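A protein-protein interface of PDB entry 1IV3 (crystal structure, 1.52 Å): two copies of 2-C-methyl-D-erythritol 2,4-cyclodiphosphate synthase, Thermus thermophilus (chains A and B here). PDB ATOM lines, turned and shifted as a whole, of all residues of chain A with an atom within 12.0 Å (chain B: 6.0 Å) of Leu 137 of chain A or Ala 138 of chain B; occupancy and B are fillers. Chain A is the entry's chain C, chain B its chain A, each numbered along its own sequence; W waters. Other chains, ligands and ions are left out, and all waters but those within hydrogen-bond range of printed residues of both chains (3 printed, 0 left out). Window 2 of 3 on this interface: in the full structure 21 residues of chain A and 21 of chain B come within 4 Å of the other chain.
The guanidinium group (NE) of Arg 11 of chain B sits at hydrogen-bond distance from the backbone carbonyl oxygen (O) of Glu 135 of chain A.
NH2 of Arg 11 of chain B lies within hydrogen-bond range of NE2 of His 141 of chain B. The backbone NH of Ala 138 of chain B lies within hydrogen-bond range of the side-chain hydroxyl of Ser 134 of chain B (3.0 Å). The side-chain hydroxyl of Ser 134 of chain A is in hydrogen-bond range of the backbone NH of Ala 138 of chain A (2.7 Å). The backbone NH (N) of Leu 137 of chain A sits at hydrogen-bond distance from the side-chain hydroxyl (OG) of Ser 134 of chain A, 3.2 Å away. OG1 of Thr 133 of chain A lies close to N of Glu 135 of chain A (3.3 Å). OG of Ser 134 of chain A sits close to N of Gly 136 of chain A (3.4 Å).
Among the printed residues, merely in contact across the chains: Ser 134 of chain A with Ser 9 of chain B (3.8 Å), Ser 134 of chain A with His 141 of chain B (3.8 Å), Glu 135 of chain A with Ser 9 of chain B (3.2 Å), Glu 135 of chain A with His 141 of chain B (2.8 Å), Gly 136 of chain A with Arg 11 of chain B (3.7 Å), Leu 137 of chain A with Ala 138 of chain B (3.7 Å), Leu 137 of chain A with His 141 of chain B (3.7 Å) and Leu 137 of chain A with Gln 143 of chain B (3.9 Å).
Thr 133 of chain A touches none of the printed residues of chain B. Of the printed residues of chain B, Glu 135 of chain A touches Ser 9, Arg 11 and His 141. Printed residues of chain B within 4 Å of Gly 136 of chain A: Arg 11 (3.7 Å). Leu 137 of chain A touches three residues of chain B. Printed residues of chain A within 4 Å of Ser 9 of chain B: Ser 134 and Glu 135. Asp 101 of chain B touches none of the printed residues of chain A. No residue of chain A comes within 4 Å of Ser 134 of chain B. Gly 136 of chain B touches none of the printed residues of chain A. Of chain A, only Leu 137 comes within 4 Å of Ala 138 of chain B. Of chain A, only Ser 134, Glu 135 and Leu 137 come within 4 Å of His 141 of chain B. Printed residues of chain A within 4 Å of Gln 143 of chain B: Leu 137 (3.9 Å). The nearest residue of chain A that does not touch Ala 138 of chain B is Ser 134 of chain A (8.3 Å). The nearest printed residue of chain B that does not touch Ser 134 of chain A is Arg 11 of chain B (6.4 Å).
Of the 14 printed residues of chain B, 5 touch a printed residue of chain A. Hydrophobic or aromatic side chains of chain B that line the printed part of chain A: Ala 138 and His 141. Hydrophobic or aromatic side chains of chain A that line the printed part of chain B: Leu 137. Among the printed residues, no Asp or Glu carboxylate lies within 4 Å of a Lys or Arg side-chain nitrogen of the other chain.
Glu 135 of chain A touches Ser 9 of chain B, but with the chains exchanged Ser 9 of chain A does not touch Glu 135 of chain B (17.4 Å). Glu 135 of chain A touches Arg 11 of chain B, but with the chains exchanged Arg 11 of chain A does not touch Glu 135 of chain B (17.1 Å). Glu 135 of chain A touches His 141 of chain B, but with the chains exchanged His 141 of chain A does not touch Glu 135 of chain B (16.9 Å). 14 positions are printed for both chains. Of the 9 pairs that touch across the chains among the printed residues, none has its exchanged pair printed and touching as well.
Water W3 lies within hydrogen-bond range of OG of Ser 9 of chain B (2.5 Å) and O of Thr 133 of chain A (2.9 Å). Water W1 bridges the backbone NH (N) of Arg 11 of chain B (2.8 Å) and the side-chain carboxylate (OE2) of Glu 135 of chain A (3.1 Å). Water W2 lies within hydrogen-bond range of the side-chain amino group of Lys 132 of chain A (3.0 Å), the side-chain carboxylate of Glu 135 of chain A (3.1 Å) and the backbone carbonyl oxygen of Ser 9 of chain B (3.1 Å).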
ATOM      1  N   GLU A   7     -16.172  12.607 -11.788  1.00  0.00           N
ATOM      2  CA  GLU A   7     -14.857  12.561 -11.161  1.00  0.00           C
ATOM      3  C   GLU A   7     -14.061  13.807 -11.525  1.00  0.00           C
ATOM      4  O   GLU A   7     -14.318  14.422 -12.554  1.00  0.00           O
ATOM      5  CB  GLU A   7     -13.995  11.378 -11.620  1.00  0.00           C
ATOM      6  CG  GLU A   7     -14.626  10.014 -11.361  1.00  0.00           C
ATOM      7  CD  GLU A   7     -13.615   8.919 -11.700  1.00  0.00           C
ATOM      8  OE1 GLU A   7     -12.401   9.157 -11.505  1.00  0.00           O
ATOM      9  OE2 GLU A   7     -14.068   7.851 -12.142  1.00  0.00           O
ATOM     10  N   SER A   9      -9.800  15.541 -11.048  1.00  0.00           N
ATOM     11  CA  SER A   9      -8.523  15.534 -10.327  1.00  0.00           C
ATOM     12  C   SER A   9      -7.623  16.631 -10.902  1.00  0.00           C
ATOM     13  O   SER A   9      -7.776  17.040 -12.053  1.00  0.00           O
ATOM     14  CB  SER A   9      -7.868  14.168 -10.414  1.00  0.00           C
ATOM     15  OG  SER A   9      -7.526  13.900 -11.754  1.00  0.00           O
ATOM     16  N   HIS A  10      -6.718  17.119 -10.056  1.00  0.00           N
ATOM     17  CA  HIS A  10      -5.785  18.171 -10.417  1.00  0.00           C
ATOM     18  C   HIS A  10      -4.469  17.988  -9.669  1.00  0.00           C
ATOM     19  O   HIS A  10      -4.387  17.554  -8.528  1.00  0.00           O
ATOM     20  CB  HIS A  10      -6.311  19.574 -10.106  1.00  0.00           C
ATOM     21  CG  HIS A  10      -7.582  19.915 -10.808  1.00  0.00           C
ATOM     22  ND1 HIS A  10      -7.611  20.274 -12.137  1.00  0.00           N
ATOM     23  CD2 HIS A  10      -8.870  19.919 -10.371  1.00  0.00           C
ATOM     24  CE1 HIS A  10      -8.878  20.498 -12.473  1.00  0.00           C
ATOM     25  NE2 HIS A  10      -9.668  20.292 -11.424  1.00  0.00           N
ATOM     26  N   ARG A  11      -3.413  18.317 -10.397  1.00  0.00           N
ATOM     27  CA  ARG A  11      -2.080  18.470  -9.852  1.00  0.00           C
ATOM     28  C   ARG A  11      -2.092  19.568  -8.797  1.00  0.00           C
ATOM     29  O   ARG A  11      -2.769  20.588  -8.942  1.00  0.00           O
ATOM     30  CB  ARG A  11      -1.140  18.850 -11.006  1.00  0.00           C
ATOM     31  CG  ARG A  11       0.307  18.419 -10.863  1.00  0.00           C
ATOM     32  CD  ARG A  11       0.978  18.463 -12.239  1.00  0.00           C
ATOM     33  NE  ARG A  11       0.914  17.164 -12.899  1.00  0.00           N
ATOM     34  CZ  ARG A  11       1.417  16.016 -12.467  1.00  0.00           C
ATOM     35  NH1 ARG A  11       2.076  15.917 -11.320  1.00  0.00           N
ATOM     36  NH2 ARG A  11       1.264  14.919 -13.203  1.00  0.00           N
ATOM     37  N   LEU A  12      -1.327  19.347  -7.742  1.00  0.00           N
ATOM     38  CA  LEU A  12      -1.202  20.344  -6.696  1.00  0.00           C
ATOM     39  C   LEU A  12       0.185  20.958  -6.721  1.00  0.00           C
ATOM     40  O   LEU A  12       1.159  20.209  -6.861  1.00  0.00           O
ATOM     41  CB  LEU A  12      -1.416  19.720  -5.316  1.00  0.00           C
ATOM     42  CG  LEU A  12      -2.817  19.153  -5.053  1.00  0.00           C
ATOM     43  CD1 LEU A  12      -2.766  18.248  -3.832  1.00  0.00           C
ATOM     44  CD2 LEU A  12      -3.792  20.312  -4.928  1.00  0.00           C
ATOM     45  N   VAL A  97     -16.223  11.583  -2.321  1.00  0.00           N
ATOM     46  CA  VAL A  97     -14.989  11.298  -1.593  1.00  0.00           C
ATOM     47  C   VAL A  97     -13.890  12.215  -2.106  1.00  0.00           C
ATOM     48  O   VAL A  97     -13.684  12.245  -3.321  1.00  0.00           O
ATOM     49  CB  VAL A  97     -14.543   9.833  -1.783  1.00  0.00           C
ATOM     50  CG1 VAL A  97     -13.315   9.492  -0.945  1.00  0.00           C
ATOM     51  CG2 VAL A  97     -15.700   8.895  -1.443  1.00  0.00           C
ATOM     52  N   LEU A  98     -13.218  12.924  -1.205  1.00  0.00           N
ATOM     53  CA  LEU A  98     -12.064  13.697  -1.637  1.00  0.00           C
ATOM     54  C   LEU A  98     -10.794  12.964  -1.206  1.00  0.00           C
ATOM     55  O   LEU A  98     -10.761  12.554  -0.033  1.00  0.00           O
ATOM     56  CB  LEU A  98     -12.069  15.112  -1.061  1.00  0.00           C
ATOM     57  CG  LEU A  98     -13.392  15.853  -1.173  1.00  0.00           C
ATOM     58  CD1 LEU A  98     -13.270  17.254  -0.584  1.00  0.00           C
ATOM     59  CD2 LEU A  98     -13.826  15.899  -2.632  1.00  0.00           C
ATOM     60  N   THR A  99      -9.835  12.839  -2.103  1.00  0.00           N
ATOM     61  CA  THR A  99      -8.557  12.218  -1.786  1.00  0.00           C
ATOM     62  C   THR A  99      -7.392  13.172  -2.021  1.00  0.00           C
ATOM     63  O   THR A  99      -7.251  13.730  -3.103  1.00  0.00           O
ATOM     64  CB  THR A  99      -8.332  10.957  -2.633  1.00  0.00           C
ATOM     65  OG1 THR A  99      -9.493  10.146  -2.446  1.00  0.00           O
ATOM     66  CG2 THR A  99      -7.168  10.118  -2.139  1.00  0.00           C
ATOM     67  N   LEU A 100      -6.588  13.320  -0.974  1.00  0.00           N
ATOM     68  CA  LEU A 100      -5.341  14.088  -1.055  1.00  0.00           C
ATOM     69  C   LEU A 100      -4.537  13.904   0.232  1.00  0.00           C
ATOM     70  O   LEU A 100      -5.100  13.733   1.326  1.00  0.00           O
ATOM     71  CB  LEU A 100      -5.586  15.561  -1.321  1.00  0.00           C
ATOM     72  CG  LEU A 100      -6.072  16.454  -0.185  1.00  0.00           C
ATOM     73  CD1 LEU A 100      -6.182  17.909  -0.637  1.00  0.00           C
ATOM     74  CD2 LEU A 100      -7.396  15.942   0.368  1.00  0.00           C
ATOM     75  N   ASP A 101      -3.220  13.930   0.073  1.00  0.00           N
ATOM     76  CA  ASP A 101      -2.352  13.600   1.206  1.00  0.00           C
ATOM     77  C   ASP A 101      -2.195  14.801   2.122  1.00  0.00           C
ATOM     78  O   ASP A 101      -1.987  14.651   3.331  1.00  0.00           O
ATOM     79  CB  ASP A 101      -1.027  13.081   0.661  1.00  0.00           C
ATOM     80  CG  ASP A 101      -1.230  11.925  -0.296  1.00  0.00           C
ATOM     81  OD1 ASP A 101      -2.367  11.426  -0.416  1.00  0.00           O
ATOM     82  OD2 ASP A 101      -0.238  11.502  -0.927  1.00  0.00           O
ATOM     83  N   ARG A 102      -2.302  16.012   1.566  1.00  0.00           N
ATOM     84  CA  ARG A 102      -2.216  17.210   2.409  1.00  0.00           C
ATOM     85  C   ARG A 102      -2.904  18.382   1.731  1.00  0.00           C
ATOM     86  O   ARG A 102      -2.927  18.432   0.495  1.00  0.00           O
ATOM     87  CB  ARG A 102      -0.750  17.533   2.734  1.00  0.00           C
ATOM     88  CG  ARG A 102       0.188  17.545   1.546  1.00  0.00           C
ATOM     89  CD  ARG A 102       1.663  17.474   1.909  1.00  0.00           C
ATOM     90  NE  ARG A 102       2.433  18.403   1.086  1.00  0.00           N
ATOM     91  CZ  ARG A 102       3.695  18.772   1.221  1.00  0.00           C
ATOM     92  NH1 ARG A 102       4.473  18.292   2.185  1.00  0.00           N
ATOM     93  NH2 ARG A 102       4.201  19.647   0.352  1.00  0.00           N
ATOM     94  N   LYS A 132     -10.133  11.113   2.329  1.00  0.00           N
ATOM     95  CA  LYS A 132      -9.111  10.073   2.344  1.00  0.00           C
ATOM     96  C   LYS A 132      -7.750  10.670   1.988  1.00  0.00           C
ATOM     97  O   LYS A 132      -7.730  11.731   1.351  1.00  0.00           O
ATOM     98  CB  LYS A 132      -9.477   8.969   1.343  1.00  0.00           C
ATOM     99  CG  LYS A 132     -10.893   8.410   1.489  1.00  0.00           C
ATOM    100  CD  LYS A 132     -10.962   7.551   2.765  1.00  0.00           C
ATOM    101  CE  LYS A 132      -9.790   6.570   2.752  1.00  0.00           C
ATOM    102  NZ  LYS A 132      -9.740   5.756   4.007  1.00  0.00           N
ATOM    103  N   THR A 133      -6.642  10.039   2.376  1.00  0.00           N
ATOM    104  CA  THR A 133      -5.334  10.290   1.780  1.00  0.00           C
ATOM    105  C   THR A 133      -5.107   9.216   0.700  1.00  0.00           C
ATOM    106  O   THR A 133      -5.843   8.237   0.745  1.00  0.00           O
ATOM    107  CB  THR A 133      -4.105  10.242   2.697  1.00  0.00           C
ATOM    108  OG1 THR A 133      -3.861   8.893   3.117  1.00  0.00           O
ATOM    109  CG2 THR A 133      -4.358  11.054   3.956  1.00  0.00           C
ATOM    110  N   SER A 134      -4.136   9.419  -0.173  1.00  0.00           N
ATOM    111  CA  SER A 134      -3.840   8.448  -1.222  1.00  0.00           C
ATOM    112  C   SER A 134      -2.891   7.357  -0.760  1.00  0.00           C
ATOM    113  O   SER A 134      -2.535   6.491  -1.558  1.00  0.00           O
ATOM    114  CB  SER A 134      -3.209   9.123  -2.448  1.00  0.00           C
ATOM    115  OG  SER A 134      -1.854   9.475  -2.199  1.00  0.00           O
ATOM    116  N   GLU A 135      -2.464   7.394   0.499  1.00  0.00           N
ATOM    117  CA  GLU A 135      -1.535   6.343   0.947  1.00  0.00           C
ATOM    118  C   GLU A 135      -0.284   6.258   0.085  1.00  0.00           C
ATOM    119  O   GLU A 135       0.307   5.196  -0.132  1.00  0.00           O
ATOM    120  CB  GLU A 135      -2.283   5.003   0.955  1.00  0.00           C
ATOM    121  CG  GLU A 135      -3.458   5.044   1.931  1.00  0.00           C
ATOM    122  CD  GLU A 135      -3.006   5.327   3.350  1.00  0.00           C
ATOM    123  OE1 GLU A 135      -3.872   5.455   4.239  1.00  0.00           O
ATOM    124  OE2 GLU A 135      -1.787   5.423   3.603  1.00  0.00           O
ATOM    125  N   GLY A 136       0.116   7.414  -0.435  1.00  0.00           N
ATOM    126  CA  GLY A 136       1.276   7.519  -1.295  1.00  0.00           C
ATOM    127  C   GLY A 136       0.971   7.133  -2.723  1.00  0.00           C
ATOM    128  O   GLY A 136       1.867   7.159  -3.568  1.00  0.00           O
ATOM    129  N   LEU A 137      -0.266   6.784  -3.042  1.00  0.00           N
ATOM    130  CA  LEU A 137      -0.648   6.525  -4.426  1.00  0.00           C
ATOM    131  C   LEU A 137      -0.598   7.792  -5.255  1.00  0.00           C
ATOM    132  O   LEU A 137      -0.258   7.813  -6.443  1.00  0.00           O
ATOM    133  CB  LEU A 137      -2.063   5.923  -4.495  1.00  0.00           C
ATOM    134  CG  LEU A 137      -2.417   5.077  -5.720  1.00  0.00           C
ATOM    135  CD1 LEU A 137      -1.221   4.253  -6.184  1.00  0.00           C
ATOM    136  CD2 LEU A 137      -3.596   4.156  -5.433  1.00  0.00           C
ATOM    137  N   ALA A 138      -0.961   8.930  -4.657  1.00  0.00           N
ATOM    138  CA  ALA A 138      -1.037  10.131  -5.497  1.00  0.00           C
ATOM    139  C   ALA A 138      -0.783  11.366  -4.644  1.00  0.00           C
ATOM    140  O   ALA A 138      -1.715  12.125  -4.392  1.00  0.00           O
ATOM    141  CB  ALA A 138      -2.381  10.211  -6.202  1.00  0.00           C
ATOM    142  N   PRO A 139       0.469  11.524  -4.224  1.00  0.00           N
ATOM    143  CA  PRO A 139       0.855  12.557  -3.273  1.00  0.00           C
ATOM    144  C   PRO A 139       0.817  13.934  -3.886  1.00  0.00           C
ATOM    145  O   PRO A 139       0.936  14.968  -3.230  1.00  0.00           O
ATOM    146  CB  PRO A 139       2.306  12.187  -2.909  1.00  0.00           C
ATOM    147  CG  PRO A 139       2.810  11.361  -4.035  1.00  0.00           C
ATOM    148  CD  PRO A 139       1.614  10.696  -4.661  1.00  0.00           C
ATOM    149  N   SER A 140       0.651  13.994  -5.219  1.00  0.00           N
ATOM    150  CA  SER A 140       0.728  15.366  -5.731  1.00  0.00           C
ATOM    151  C   SER A 140      -0.541  15.770  -6.444  1.00  0.00           C
ATOM    152  O   SER A 140      -0.579  16.733  -7.214  1.00  0.00           O
ATOM    153  CB  SER A 140       1.982  15.456  -6.618  1.00  0.00           C
ATOM    154  OG  SER A 140       3.116  15.501  -5.745  1.00  0.00           O
ATOM    155  N   HIS A 141      -1.617  15.017  -6.172  1.00  0.00           N
ATOM    156  CA  HIS A 141      -2.895  15.371  -6.777  1.00  0.00           C
ATOM    157  C   HIS A 141      -4.002  15.489  -5.732  1.00  0.00           C
ATOM    158  O   HIS A 141      -3.977  14.858  -4.684  1.00  0.00           O
ATOM    159  CB  HIS A 141      -3.342  14.336  -7.816  1.00  0.00           C
ATOM    160  CG  HIS A 141      -2.497  14.385  -9.055  1.00  0.00           C
ATOM    161  ND1 HIS A 141      -2.978  14.726 -10.300  1.00  0.00           N
ATOM    162  CD2 HIS A 141      -1.179  14.108  -9.219  1.00  0.00           C
ATOM    163  CE1 HIS A 141      -1.996  14.666 -11.184  1.00  0.00           C
ATOM    164  NE2 HIS A 141      -0.896  14.297 -10.552  1.00  0.00           N
ATOM    165  N   VAL A 142      -4.995  16.293  -6.078  1.00  0.00           N
ATOM    166  CA  VAL A 142      -6.267  16.125  -5.353  1.00  0.00           C
ATOM    167  C   VAL A 142      -7.234  15.380  -6.272  1.00  0.00           C
ATOM    168  O   VAL A 142      -7.205  15.601  -7.491  1.00  0.00           O
ATOM    169  CB  VAL A 142      -6.849  17.460  -4.905  1.00  0.00           C
ATOM    170  CG1 VAL A 142      -6.894  18.458  -6.035  1.00  0.00           C
ATOM    171  CG2 VAL A 142      -8.254  17.221  -4.327  1.00  0.00           C
ATOM    172  N   GLN A 143      -8.063  14.508  -5.703  1.00  0.00           N
ATOM    173  CA  GLN A 143      -9.013  13.722  -6.478  1.00  0.00           C
ATOM    174  C   GLN A 143     -10.392  13.775  -5.838  1.00  0.00           C
ATOM    175  O   GLN A 143     -10.485  13.842  -4.608  1.00  0.00           O
ATOM    176  CB  GLN A 143      -8.626  12.247  -6.575  1.00  0.00           C
ATOM    177  CG  GLN A 143      -7.217  12.010  -7.092  1.00  0.00           C
ATOM    178  CD  GLN A 143      -6.811  10.561  -6.877  1.00  0.00           C
ATOM    179  OE1 GLN A 143      -6.060  10.240  -5.951  1.00  0.00           O
ATOM    180  NE2 GLN A 143      -7.329   9.694  -7.738  1.00  0.00           N
ATOM    181  N   ARG A 145     -14.522  12.089  -6.378  1.00  0.00           N
ATOM    182  CA  ARG A 145     -15.461  11.205  -7.085  1.00  0.00           C
ATOM    183  C   ARG A 145     -16.825  11.357  -6.416  1.00  0.00           C
ATOM    184  O   ARG A 145     -16.911  11.301  -5.194  1.00  0.00           O
ATOM    185  CB  ARG A 145     -14.998   9.746  -7.116  1.00  0.00           C
ATOM    186  CG  ARG A 145     -13.699   9.597  -7.913  1.00  0.00           C
ATOM    187  CD  ARG A 145     -13.293   8.150  -8.186  1.00  0.00           C
ATOM    188  NE  ARG A 145     -11.927   8.192  -8.720  1.00  0.00           N
ATOM    189  CZ  ARG A 145     -10.822   8.155  -7.992  1.00  0.00           C
ATOM    190  NH1 ARG A 145     -10.798   8.057  -6.669  1.00  0.00           N
ATOM    191  NH2 ARG A 145      -9.671   8.211  -8.657  1.00  0.00           N
ATOM    192  N   SER B   9      -7.994   2.940   0.328  1.00  0.00           N
ATOM    193  CA  SER B   9      -6.801   2.321  -0.257  1.00  0.00           C
ATOM    194  C   SER B   9      -5.763   2.083   0.835  1.00  0.00           C
ATOM    195  O   SER B   9      -5.755   2.807   1.828  1.00  0.00           O
ATOM    196  CB  SER B   9      -6.244   3.191  -1.381  1.00  0.00           C
ATOM    197  OG  SER B   9      -5.614   4.351  -0.853  1.00  0.00           O
ATOM    198  N   ARG B  11      -1.446   0.814   1.208  1.00  0.00           N
ATOM    199  CA  ARG B  11      -0.172   0.335   0.703  1.00  0.00           C
ATOM    200  C   ARG B  11      -0.106  -1.145   1.074  1.00  0.00           C
ATOM    201  O   ARG B  11      -0.478  -1.563   2.169  1.00  0.00           O
ATOM    202  CB  ARG B  11       0.974   1.113   1.309  1.00  0.00           C
ATOM    203  CG  ARG B  11       2.310   1.105   0.607  1.00  0.00           C
ATOM    204  CD  ARG B  11       3.112   2.354   0.996  1.00  0.00           C
ATOM    205  NE  ARG B  11       3.064   3.350  -0.073  1.00  0.00           N
ATOM    206  CZ  ARG B  11       3.493   3.154  -1.316  1.00  0.00           C
ATOM    207  NH1 ARG B  11       4.019   1.993  -1.685  1.00  0.00           N
ATOM    208  NH2 ARG B  11       3.397   4.134  -2.211  1.00  0.00           N
ATOM    209  N   LEU B 100      -6.544  -4.881  -6.938  1.00  0.00           N
ATOM    210  CA  LEU B 100      -5.194  -5.207  -6.466  1.00  0.00           C
ATOM    211  C   LEU B 100      -4.556  -6.192  -7.445  1.00  0.00           C
ATOM    212  O   LEU B 100      -5.258  -6.995  -8.073  1.00  0.00           O
ATOM    213  CB  LEU B 100      -5.215  -5.756  -5.044  1.00  0.00           C
ATOM    214  CG  LEU B 100      -5.685  -7.192  -4.812  1.00  0.00           C
ATOM    215  CD1 LEU B 100      -5.615  -7.564  -3.330  1.00  0.00           C
ATOM    216  CD2 LEU B 100      -7.094  -7.399  -5.326  1.00  0.00           C
ATOM    217  N   ASP B 101      -3.238  -6.106  -7.604  1.00  0.00           N
ATOM    218  CA  ASP B 101      -2.579  -6.943  -8.612  1.00  0.00           C
ATOM    219  C   ASP B 101      -2.325  -8.350  -8.103  1.00  0.00           C
ATOM    220  O   ASP B 101      -2.233  -9.289  -8.902  1.00  0.00           O
ATOM    221  CB  ASP B 101      -1.285  -6.255  -9.078  1.00  0.00           C
ATOM    222  CG  ASP B 101      -1.581  -4.940  -9.773  1.00  0.00           C
ATOM    223  OD1 ASP B 101      -2.704  -4.406  -9.656  1.00  0.00           O
ATOM    224  OD2 ASP B 101      -0.696  -4.414 -10.485  1.00  0.00           O
ATOM    225  N   SER B 134      -4.849  -3.707 -11.177  1.00  0.00           N
ATOM    226  CA  SER B 134      -4.617  -2.316 -11.559  1.00  0.00           C
ATOM    227  C   SER B 134      -3.957  -2.211 -12.928  1.00  0.00           C
ATOM    228  O   SER B 134      -3.710  -1.108 -13.403  1.00  0.00           O
ATOM    229  CB  SER B 134      -3.695  -1.628 -10.544  1.00  0.00           C
ATOM    230  OG  SER B 134      -2.361  -2.116 -10.675  1.00  0.00           O
ATOM    231  N   GLU B 135      -3.667  -3.367 -13.524  1.00  0.00           N
ATOM    232  CA  GLU B 135      -2.906  -3.346 -14.781  1.00  0.00           C
ATOM    233  C   GLU B 135      -1.627  -2.554 -14.585  1.00  0.00           C
ATOM    234  O   GLU B 135      -1.156  -1.823 -15.469  1.00  0.00           O
ATOM    235  CB  GLU B 135      -3.749  -2.742 -15.898  1.00  0.00           C
ATOM    236  CG  GLU B 135      -4.967  -3.526 -16.323  1.00  0.00           C
ATOM    237  CD  GLU B 135      -4.674  -4.914 -16.846  1.00  0.00           C
ATOM    238  OE1 GLU B 135      -5.557  -5.791 -16.704  1.00  0.00           O
ATOM    239  OE2 GLU B 135      -3.580  -5.149 -17.387  1.00  0.00           O
ATOM    240  N   GLY B 136      -1.032  -2.659 -13.393  1.00  0.00           N
ATOM    241  CA  GLY B 136       0.220  -1.965 -13.153  1.00  0.00           C
ATOM    242  C   GLY B 136       0.090  -0.499 -12.841  1.00  0.00           C
ATOM    243  O   GLY B 136       1.088   0.196 -12.628  1.00  0.00           O
ATOM    244  N   LEU B 137      -1.154  -0.016 -12.798  1.00  0.00           N
ATOM    245  CA  LEU B 137      -1.354   1.383 -12.416  1.00  0.00           C
ATOM    246  C   LEU B 137      -0.937   1.600 -10.963  1.00  0.00           C
ATOM    247  O   LEU B 137      -0.298   2.597 -10.620  1.00  0.00           O
ATOM    248  CB  LEU B 137      -2.815   1.731 -12.656  1.00  0.00           C
ATOM    249  CG  LEU B 137      -3.237   3.195 -12.564  1.00  0.00           C
ATOM    250  CD1 LEU B 137      -2.053   4.128 -12.734  1.00  0.00           C
ATOM    251  CD2 LEU B 137      -4.305   3.483 -13.611  1.00  0.00           C
ATOM    252  N   ALA B 138      -1.292   0.656 -10.094  1.00  0.00           N
ATOM    253  CA  ALA B 138      -1.085   0.725  -8.655  1.00  0.00           C
ATOM    254  C   ALA B 138      -0.720  -0.657  -8.133  1.00  0.00           C
ATOM    255  O   ALA B 138      -1.519  -1.305  -7.464  1.00  0.00           O
ATOM    256  CB  ALA B 138      -2.335   1.240  -7.948  1.00  0.00           C
ATOM    257  N   PRO B 139       0.468  -1.154  -8.453  1.00  0.00           N
ATOM    258  CA  PRO B 139       0.813  -2.554  -8.175  1.00  0.00           C
ATOM    259  C   PRO B 139       1.108  -2.841  -6.720  1.00  0.00           C
ATOM    260  O   PRO B 139       1.308  -3.975  -6.304  1.00  0.00           O
ATOM    261  CB  PRO B 139       2.126  -2.739  -8.963  1.00  0.00           C
ATOM    262  CG  PRO B 139       2.738  -1.374  -8.881  1.00  0.00           C
ATOM    263  CD  PRO B 139       1.580  -0.426  -9.104  1.00  0.00           C
ATOM    264  N   SER B 140       1.158  -1.787  -5.910  1.00  0.00           N
ATOM    265  CA  SER B 140       1.469  -2.037  -4.519  1.00  0.00           C
ATOM    266  C   SER B 140       0.390  -1.505  -3.582  1.00  0.00           C
ATOM    267  O   SER B 140       0.678  -1.257  -2.412  1.00  0.00           O
ATOM    268  CB  SER B 140       2.839  -1.411  -4.211  1.00  0.00           C
ATOM    269  OG  SER B 140       3.862  -2.177  -4.838  1.00  0.00           O
ATOM    270  N   HIS B 141      -0.843  -1.340  -4.065  1.00  0.00           N
ATOM    271  CA  HIS B 141      -1.941  -0.956  -3.182  1.00  0.00           C
ATOM    272  C   HIS B 141      -3.135  -1.885  -3.402  1.00  0.00           C
ATOM    273  O   HIS B 141      -3.302  -2.460  -4.477  1.00  0.00           O
ATOM    274  CB  HIS B 141      -2.413   0.474  -3.405  1.00  0.00           C
ATOM    275  CG  HIS B 141      -1.439   1.539  -3.020  1.00  0.00           C
ATOM    276  ND1 HIS B 141      -1.667   2.405  -1.982  1.00  0.00           N
ATOM    277  CD2 HIS B 141      -0.235   1.884  -3.553  1.00  0.00           C
ATOM    278  CE1 HIS B 141      -0.635   3.233  -1.882  1.00  0.00           C
ATOM    279  NE2 HIS B 141       0.239   2.942  -2.815  1.00  0.00           N
ATOM    280  N   VAL B 142      -3.946  -2.002  -2.364  1.00  0.00           N
ATOM    281  CA  VAL B 142      -5.291  -2.564  -2.512  1.00  0.00           C
ATOM    282  C   VAL B 142      -6.252  -1.376  -2.545  1.00  0.00           C
ATOM    283  O   VAL B 142      -6.094  -0.475  -1.698  1.00  0.00           O
ATOM    284  CB  VAL B 142      -5.644  -3.551  -1.403  1.00  0.00           C
ATOM    285  CG1 VAL B 142      -5.422  -2.956  -0.001  1.00  0.00           C
ATOM    286  CG2 VAL B 142      -7.082  -4.028  -1.562  1.00  0.00           C
ATOM    287  N   GLN B 143      -7.189  -1.338  -3.493  1.00  0.00           N
ATOM    288  CA  GLN B 143      -8.123  -0.212  -3.514  1.00  0.00           C
ATOM    289  C   GLN B 143      -9.549  -0.756  -3.424  1.00  0.00           C
ATOM    290  O   GLN B 143      -9.801  -1.836  -3.971  1.00  0.00           O
ATOM    291  CB  GLN B 143      -7.994   0.615  -4.776  1.00  0.00           C
ATOM    292  CG  GLN B 143      -6.580   1.104  -5.060  1.00  0.00           C
ATOM    293  CD  GLN B 143      -6.399   1.627  -6.478  1.00  0.00           C
ATOM    294  OE1 GLN B 143      -5.754   1.017  -7.335  1.00  0.00           O
ATOM    295  NE2 GLN B 143      -6.990   2.787  -6.744  1.00  0.00           N
HETATM  296  O   HOH W   1      -1.446   2.309   3.594  1.00  0.00           O
HETATM  297  O   HOH W   2      -6.854   5.271   3.407  1.00  0.00           O
HETATM  298  O   HOH W   3      -6.904   5.565   0.907  1.00  0.00           O
